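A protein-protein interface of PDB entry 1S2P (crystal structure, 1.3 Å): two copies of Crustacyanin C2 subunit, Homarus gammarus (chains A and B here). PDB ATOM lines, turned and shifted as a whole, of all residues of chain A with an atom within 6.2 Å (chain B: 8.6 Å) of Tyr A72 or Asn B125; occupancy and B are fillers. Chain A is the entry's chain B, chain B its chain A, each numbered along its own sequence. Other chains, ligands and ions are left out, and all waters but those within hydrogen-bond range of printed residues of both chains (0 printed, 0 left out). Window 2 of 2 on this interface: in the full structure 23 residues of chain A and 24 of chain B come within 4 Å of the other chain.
O of Asn A43 is in hydrogen-bond range of ND2 of Asn B125 (2.8 Å). The backbone NH (N) of Asn B125 lies within hydrogen-bond range of the backbone carbonyl oxygen (O) of Pro A44, at 2.8 Å. ND2 of Asn B125 sits at hydrogen-bond distance from O of Gln A46 (2.9 Å).
OD1 of Asn A43 sits at hydrogen-bond distance from N of Tyr A45 (2.8 Å). The side-chain amide oxygen (OD1) of Asn A43 lies within hydrogen-bond range of the backbone NH (N) of Gln A46 (3.1 Å). The backbone NH of Ile A48 is in hydrogen-bond range of the side-chain amide oxygen of Gln A46, at 3.0 Å.
Among the printed residues, merely in contact across the chains: Pro A44 with Tyr B124, Pro A44 with Phe B126, Tyr A45 with Tyr B124, Tyr A45 with Asn B125, Leu A47 with Asn B125 and Tyr A72 with Asn B125.
Of the printed residues of chain B, Asn A43 touches Asn B125. Of the printed residues of chain B, Pro A44 touches Tyr B124 (3.2 Å), Asn B125 (2.8 Å) and Phe B126 (3.9 Å). Printed residues of chain B within 4 Å of Tyr A45: Tyr B124 and Asn B125. Of the printed residues of chain B, Gln A46 touches Asn B125 (2.9 Å). Glu A49 touches none of the printed residues of chain B. Ile A70 touches none of the printed residues of chain B. Ala A71 touches none of the printed residues of chain B. Tyr A72 touches one residue of chain B. Of the printed residues of chain A, Tyr B124 touches Pro A44 and Tyr A45. Of chain A, only Asn A43, Pro A44, Tyr A45, Gln A46, Leu A47 and Tyr A72 come within 4 Å of Asn B125. The nearest printed residue of chain A that does not touch Asn B125 is Ile A48 (6.2 Å). The nearest printed residue of chain B that does not touch Tyr A45 is Ile B122 (4.004 Å).
Printed residues of chain B that touch a printed residue of chain A: Tyr B124, Asn B125 and Phe B126. Of the 13 printed residues of chain A, 6 touch a printed residue of chain B. Among the printed residues, 9 pairs touch across the chains.
No position is printed for both chains.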
ATOM      1  N   ASN A  43      26.859  13.634  14.983  1.00  0.00           N
ATOM      2  CA  ASN A  43      28.060  13.702  15.811  1.00  0.00           C
ATOM      3  C   ASN A  43      27.757  13.059  17.154  1.00  0.00           C
ATOM      4  O   ASN A  43      26.955  13.593  17.909  1.00  0.00           O
ATOM      5  CB  ASN A  43      28.447  15.178  15.974  1.00  0.00           C
ATOM      6  CG  ASN A  43      29.785  15.366  16.623  1.00  0.00           C
ATOM      7  OD1 ASN A  43      30.085  14.700  17.618  1.00  0.00           O
ATOM      8  ND2 ASN A  43      30.596  16.289  16.099  1.00  0.00           N
ATOM      9  N   PRO A  44      28.338  11.888  17.435  1.00  0.00           N
ATOM     10  CA  PRO A  44      28.098  11.157  18.683  1.00  0.00           C
ATOM     11  C   PRO A  44      28.920  11.722  19.862  1.00  0.00           C
ATOM     12  O   PRO A  44      28.825  11.172  20.956  1.00  0.00           O
ATOM     13  CB  PRO A  44      28.565   9.736  18.312  1.00  0.00           C
ATOM     14  CG  PRO A  44      29.786  10.020  17.524  1.00  0.00           C
ATOM     15  CD  PRO A  44      29.283  11.135  16.580  1.00  0.00           C
ATOM     16  N   TYR A  45      29.691  12.786  19.649  1.00  0.00           N
ATOM     17  CA  TYR A  45      30.574  13.321  20.686  1.00  0.00           C
ATOM     18  C   TYR A  45      29.999  14.583  21.306  1.00  0.00           C
ATOM     19  O   TYR A  45      30.129  14.786  22.511  1.00  0.00           O
ATOM     20  CB  TYR A  45      31.984  13.558  20.145  1.00  0.00           C
ATOM     21  CG  TYR A  45      32.557  12.320  19.519  1.00  0.00           C
ATOM     22  CD1 TYR A  45      32.836  12.280  18.166  1.00  0.00           C
ATOM     23  CD2 TYR A  45      32.831  11.185  20.282  1.00  0.00           C
ATOM     24  CE1 TYR A  45      33.354  11.158  17.573  1.00  0.00           C
ATOM     25  CE2 TYR A  45      33.354  10.040  19.695  1.00  0.00           C
ATOM     26  CZ  TYR A  45      33.610  10.035  18.331  1.00  0.00           C
ATOM     27  OH  TYR A  45      34.133   8.915  17.715  1.00  0.00           O
ATOM     28  N   GLN A  46      29.306  15.394  20.511  1.00  0.00           N
ATOM     29  CA  GLN A  46      28.755  16.681  20.955  1.00  0.00           C
ATOM     30  C   GLN A  46      27.713  16.513  22.058  1.00  0.00           C
ATOM     31  O   GLN A  46      26.653  15.967  21.815  1.00  0.00           O
ATOM     32  CB  GLN A  46      28.178  17.395  19.722  1.00  0.00           C
ATOM     33  CG  GLN A  46      27.260  18.600  19.947  1.00  0.00           C
ATOM     34  CD  GLN A  46      27.931  19.770  20.585  1.00  0.00           C
ATOM     35  OE1 GLN A  46      28.253  19.734  21.773  1.00  0.00           O
ATOM     36  NE2 GLN A  46      28.098  20.853  19.815  1.00  0.00           N
ATOM     37  N   LEU A  47      28.013  17.032  23.252  1.00  0.00           N
ATOM     38  CA  LEU A  47      27.142  16.875  24.406  1.00  0.00           C
ATOM     39  C   LEU A  47      26.033  17.920  24.485  1.00  0.00           C
ATOM     40  O   LEU A  47      25.076  17.743  25.228  1.00  0.00           O
ATOM     41  CB  LEU A  47      27.965  16.909  25.705  1.00  0.00           C
ATOM     42  CG  LEU A  47      29.035  15.823  25.793  1.00  0.00           C
ATOM     43  CD1 LEU A  47      29.851  15.929  27.107  1.00  0.00           C
ATOM     44  CD2 LEU A  47      28.380  14.472  25.698  1.00  0.00           C
ATOM     45  N   ILE A  48      26.179  19.022  23.749  1.00  0.00           N
ATOM     46  CA  ILE A  48      25.190  20.099  23.756  1.00  0.00           C
ATOM     47  C   ILE A  48      24.249  19.904  22.566  1.00  0.00           C
ATOM     48  O   ILE A  48      24.684  19.994  21.411  1.00  0.00           O
ATOM     49  CB  ILE A  48      25.889  21.477  23.722  1.00  0.00           C
ATOM     50  CG1 ILE A  48      27.014  21.550  24.759  1.00  0.00           C
ATOM     51  CG2 ILE A  48      24.859  22.619  23.916  1.00  0.00           C
ATOM     52  CD1 ILE A  48      27.847  22.814  24.629  1.00  0.00           C
ATOM     53  N   GLU A  49      22.980  19.632  22.850  1.00  0.00           N
ATOM     54  CA  GLU A  49      21.998  19.345  21.801  1.00  0.00           C
ATOM     55  C   GLU A  49      21.391  20.607  21.193  1.00  0.00           C
ATOM     56  O   GLU A  49      21.292  20.716  19.959  1.00  0.00           O
ATOM     57  CB  GLU A  49      20.865  18.450  22.327  1.00  0.00           C
ATOM     58  CG  GLU A  49      19.795  18.125  21.278  1.00  0.00           C
ATOM     59  CD  GLU A  49      18.624  17.291  21.772  1.00  0.00           C
ATOM     60  OE1 GLU A  49      17.965  16.636  20.921  1.00  0.00           O
ATOM     61  OE2 GLU A  49      18.345  17.291  22.985  1.00  0.00           O
ATOM     62  N   ILE A  70      21.770  23.618  25.794  1.00  0.00           N
ATOM     63  CA  ILE A  70      20.983  22.619  26.523  1.00  0.00           C
ATOM     64  C   ILE A  70      21.462  21.209  26.165  1.00  0.00           C
ATOM     65  O   ILE A  70      21.542  20.873  24.985  1.00  0.00           O
ATOM     66  CB  ILE A  70      19.458  22.777  26.217  1.00  0.00           C
ATOM     67  CG1 ILE A  70      19.003  24.232  26.362  1.00  0.00           C
ATOM     68  CG2 ILE A  70      18.623  21.899  27.145  1.00  0.00           C
ATOM     69  CD1 ILE A  70      17.600  24.505  25.852  1.00  0.00           C
ATOM     70  N   ALA A  71      21.819  20.427  27.186  1.00  0.00           N
ATOM     71  CA  ALA A  71      22.329  19.072  27.031  1.00  0.00           C
ATOM     72  C   ALA A  71      21.182  18.148  26.649  1.00  0.00           C
ATOM     73  O   ALA A  71      20.017  18.560  26.689  1.00  0.00           O
ATOM     74  CB  ALA A  71      22.962  18.630  28.314  1.00  0.00           C
ATOM     75  N   TYR A  72      21.503  16.903  26.298  1.00  0.00           N
ATOM     76  CA  TYR A  72      20.480  15.948  25.838  1.00  0.00           C
ATOM     77  C   TYR A  72      19.463  15.579  26.949  1.00  0.00           C
ATOM     78  O   TYR A  72      18.351  15.106  26.675  1.00  0.00           O
ATOM     79  CB  TYR A  72      21.148  14.704  25.209  1.00  0.00           C
ATOM     80  CG  TYR A  72      21.671  14.968  23.798  1.00  0.00           C
ATOM     81  CD1 TYR A  72      22.935  15.499  23.567  1.00  0.00           C
ATOM     82  CD2 TYR A  72      20.856  14.735  22.705  1.00  0.00           C
ATOM     83  CE1 TYR A  72      23.378  15.765  22.266  1.00  0.00           C
ATOM     84  CE2 TYR A  72      21.277  14.988  21.421  1.00  0.00           C
ATOM     85  CZ  TYR A  72      22.538  15.504  21.195  1.00  0.00           C
ATOM     86  OH  TYR A  72      22.948  15.776  19.902  1.00  0.00           O
ATOM     87  N   ASP A  73      19.843  15.822  28.195  1.00  0.00           N
ATOM     88  CA  ASP A  73      18.963  15.547  29.330  1.00  0.00           C
ATOM     89  C   ASP A  73      18.081  16.737  29.690  1.00  0.00           C
ATOM     90  O   ASP A  73      17.318  16.674  30.657  1.00  0.00           O
ATOM     91  CB  ASP A  73      19.771  15.072  30.557  1.00  0.00           C
ATOM     92  CG  ASP A  73      20.653  16.155  31.175  1.00  0.00           C
ATOM     93  OD1 ASP A  73      20.764  17.277  30.640  1.00  0.00           O
ATOM     94  OD2 ASP A  73      21.283  15.948  32.242  1.00  0.00           O
ATOM     95  N   GLY A  74      18.190  17.836  28.949  1.00  0.00           N
ATOM     96  CA  GLY A  74      17.355  18.996  29.196  1.00  0.00           C
ATOM     97  C   GLY A  74      17.954  20.052  30.118  1.00  0.00           C
ATOM     98  O   GLY A  74      17.377  21.109  30.304  1.00  0.00           O
ATOM     99  N   ASN A  75      19.119  19.776  30.678  1.00  0.00           N
ATOM    100  CA  ASN A  75      19.784  20.711  31.569  1.00  0.00           C
ATOM    101  C   ASN A  75      20.748  21.643  30.848  1.00  0.00           C
ATOM    102  O   ASN A  75      21.329  21.286  29.836  1.00  0.00           O
ATOM    103  CB  ASN A  75      20.539  19.947  32.648  1.00  0.00           C
ATOM    104  CG  ASN A  75      19.608  19.339  33.670  1.00  0.00           C
ATOM    105  OD1 ASN A  75      18.753  20.029  34.226  1.00  0.00           O
ATOM    106  ND2 ASN A  75      19.743  18.035  33.900  1.00  0.00           N
ATOM    107  N   ILE B 122      36.588   7.316  25.832  1.00  0.00           N
ATOM    108  CA  ILE B 122      35.832   8.441  25.261  1.00  0.00           C
ATOM    109  C   ILE B 122      34.323   8.202  25.440  1.00  0.00           C
ATOM    110  O   ILE B 122      33.826   7.129  25.187  1.00  0.00           O
ATOM    111  CB  ILE B 122      36.158   8.628  23.754  1.00  0.00           C
ATOM    112  CG1 ILE B 122      37.670   8.819  23.519  1.00  0.00           C
ATOM    113  CG2 ILE B 122      35.328   9.772  23.168  1.00  0.00           C
ATOM    114  CD1 ILE B 122      38.354   7.514  23.248  1.00  0.00           C
ATOM    115  N   ASP B 123      33.611   9.224  25.889  1.00  0.00           N
ATOM    116  CA  ASP B 123      32.177   9.154  26.100  1.00  0.00           C
ATOM    117  C   ASP B 123      31.395   9.634  24.882  1.00  0.00           C
ATOM    118  O   ASP B 123      31.805  10.553  24.197  1.00  0.00           O
ATOM    119  CB  ASP B 123      31.804  10.073  27.252  1.00  0.00           C
ATOM    120  CG  ASP B 123      32.160   9.497  28.613  1.00  0.00           C
ATOM    121  OD1 ASP B 123      31.647   8.408  29.009  1.00  0.00           O
ATOM    122  OD2 ASP B 123      32.927  10.117  29.385  1.00  0.00           O
ATOM    123  N   TYR B 124      30.258   9.000  24.632  1.00  0.00           N
ATOM    124  CA  TYR B 124      29.318   9.413  23.580  1.00  0.00           C
ATOM    125  C   TYR B 124      28.119  10.139  24.197  1.00  0.00           C
ATOM    126  O   TYR B 124      27.823  10.017  25.385  1.00  0.00           O
ATOM    127  CB  TYR B 124      28.841   8.216  22.760  1.00  0.00           C
ATOM    128  CG  TYR B 124      29.911   7.424  22.034  1.00  0.00           C
ATOM    129  CD1 TYR B 124      30.175   6.107  22.385  1.00  0.00           C
ATOM    130  CD2 TYR B 124      30.575   7.950  20.947  1.00  0.00           C
ATOM    131  CE1 TYR B 124      31.126   5.353  21.715  1.00  0.00           C
ATOM    132  CE2 TYR B 124      31.524   7.200  20.262  1.00  0.00           C
ATOM    133  CZ  TYR B 124      31.786   5.901  20.657  1.00  0.00           C
ATOM    134  OH  TYR B 124      32.737   5.143  19.998  1.00  0.00           O
ATOM    135  N   ASN B 125      27.418  10.911  23.370  1.00  0.00           N
ATOM    136  CA  ASN B 125      26.244  11.654  23.812  1.00  0.00           C
ATOM    137  C   ASN B 125      24.962  10.818  24.006  1.00  0.00           C
ATOM    138  O   ASN B 125      23.982  11.305  24.555  1.00  0.00           O
ATOM    139  CB  ASN B 125      26.051  12.870  22.901  1.00  0.00           C
ATOM    140  CG  ASN B 125      25.745  12.493  21.474  1.00  0.00           C
ATOM    141  OD1 ASN B 125      25.396  11.345  21.182  1.00  0.00           O
ATOM    142  ND2 ASN B 125      25.940  13.445  20.560  1.00  0.00           N
ATOM    143  N   PHE B 126      25.020   9.548  23.622  1.00  0.00           N
ATOM    144  CA  PHE B 126      23.892   8.615  23.770  1.00  0.00           C
ATOM    145  C   PHE B 126      24.031   7.661  24.960  1.00  0.00           C
ATOM    146  O   PHE B 126      23.275   6.715  25.060  1.00  0.00           O
ATOM    147  CB  PHE B 126      23.563   7.855  22.451  1.00  0.00           C
ATOM    148  CG  PHE B 126      24.706   7.105  21.840  1.00  0.00           C
ATOM    149  CD1 PHE B 126      24.936   5.785  22.154  1.00  0.00           C
ATOM    150  CD2 PHE B 126      25.503   7.696  20.888  1.00  0.00           C
ATOM    151  CE1 PHE B 126      25.966   5.101  21.572  1.00  0.00           C
ATOM    152  CE2 PHE B 126      26.554   7.022  20.330  1.00  0.00           C
ATOM    153  CZ  PHE B 126      26.775   5.716  20.662  1.00  0.00           C
ATOM    154  N   GLY B 127      24.970   7.921  25.860  1.00  0.00           N
ATOM    155  CA  GLY B 127      25.057   7.151  27.097  1.00  0.00           C
ATOM    156  C   GLY B 127      25.876   5.872  27.056  1.00  0.00           C
ATOM    157  O   GLY B 127      25.678   4.955  27.877  1.00  0.00           O
ATOM    158  N   TYR B 128      26.728   5.780  26.048  1.00  0.00           N
ATOM    159  CA  TYR B 128      27.718   4.706  25.888  1.00  0.00           C
ATOM    160  C   TYR B 128      29.120   5.362  25.903  1.00  0.00           C
ATOM    161  O   TYR B 128      29.255   6.576  25.957  1.00  0.00           O
ATOM    162  CB  TYR B 128      27.525   3.945  24.566  1.00  0.00           C
ATOM    163  CG  TYR B 128      26.438   2.865  24.529  1.00  0.00           C
ATOM    164  CD1 TYR B 128      26.745   1.595  24.082  1.00  0.00           C
ATOM    165  CD2 TYR B 128      25.113   3.133  24.894  1.00  0.00           C
ATOM    166  CE1 TYR B 128      25.784   0.612  24.020  1.00  0.00           C
ATOM    167  CE2 TYR B 128      24.153   2.148  24.819  1.00  0.00           C
ATOM    168  CZ  TYR B 128      24.495   0.904  24.375  1.00  0.00           C
ATOM    169  OH  TYR B 128      23.528  -0.091  24.311  1.00  0.00           O
ATOM    170  N   HIS B 129      30.139   4.521  25.889  1.00  0.00           N
ATOM    171  CA  HIS B 129      31.539   4.940  25.769  1.00  0.00           C
ATOM    172  C   HIS B 129      32.291   3.959  24.904  1.00  0.00           C
ATOM    173  O   HIS B 129      31.821   2.868  24.610  1.00  0.00           O
ATOM    174  CB  HIS B 129      32.263   5.004  27.140  1.00  0.00           C
ATOM    175  CG  HIS B 129      32.329   3.701  27.881  1.00  0.00           C
ATOM    176  ND1 HIS B 129      33.452   2.892  27.964  1.00  0.00           N
ATOM    177  CD2 HIS B 129      31.376   3.096  28.631  1.00  0.00           C
ATOM    178  CE1 HIS B 129      33.159   1.830  28.699  1.00  0.00           C
ATOM    179  NE2 HIS B 129      31.913   1.940  29.126  1.00  0.00           N
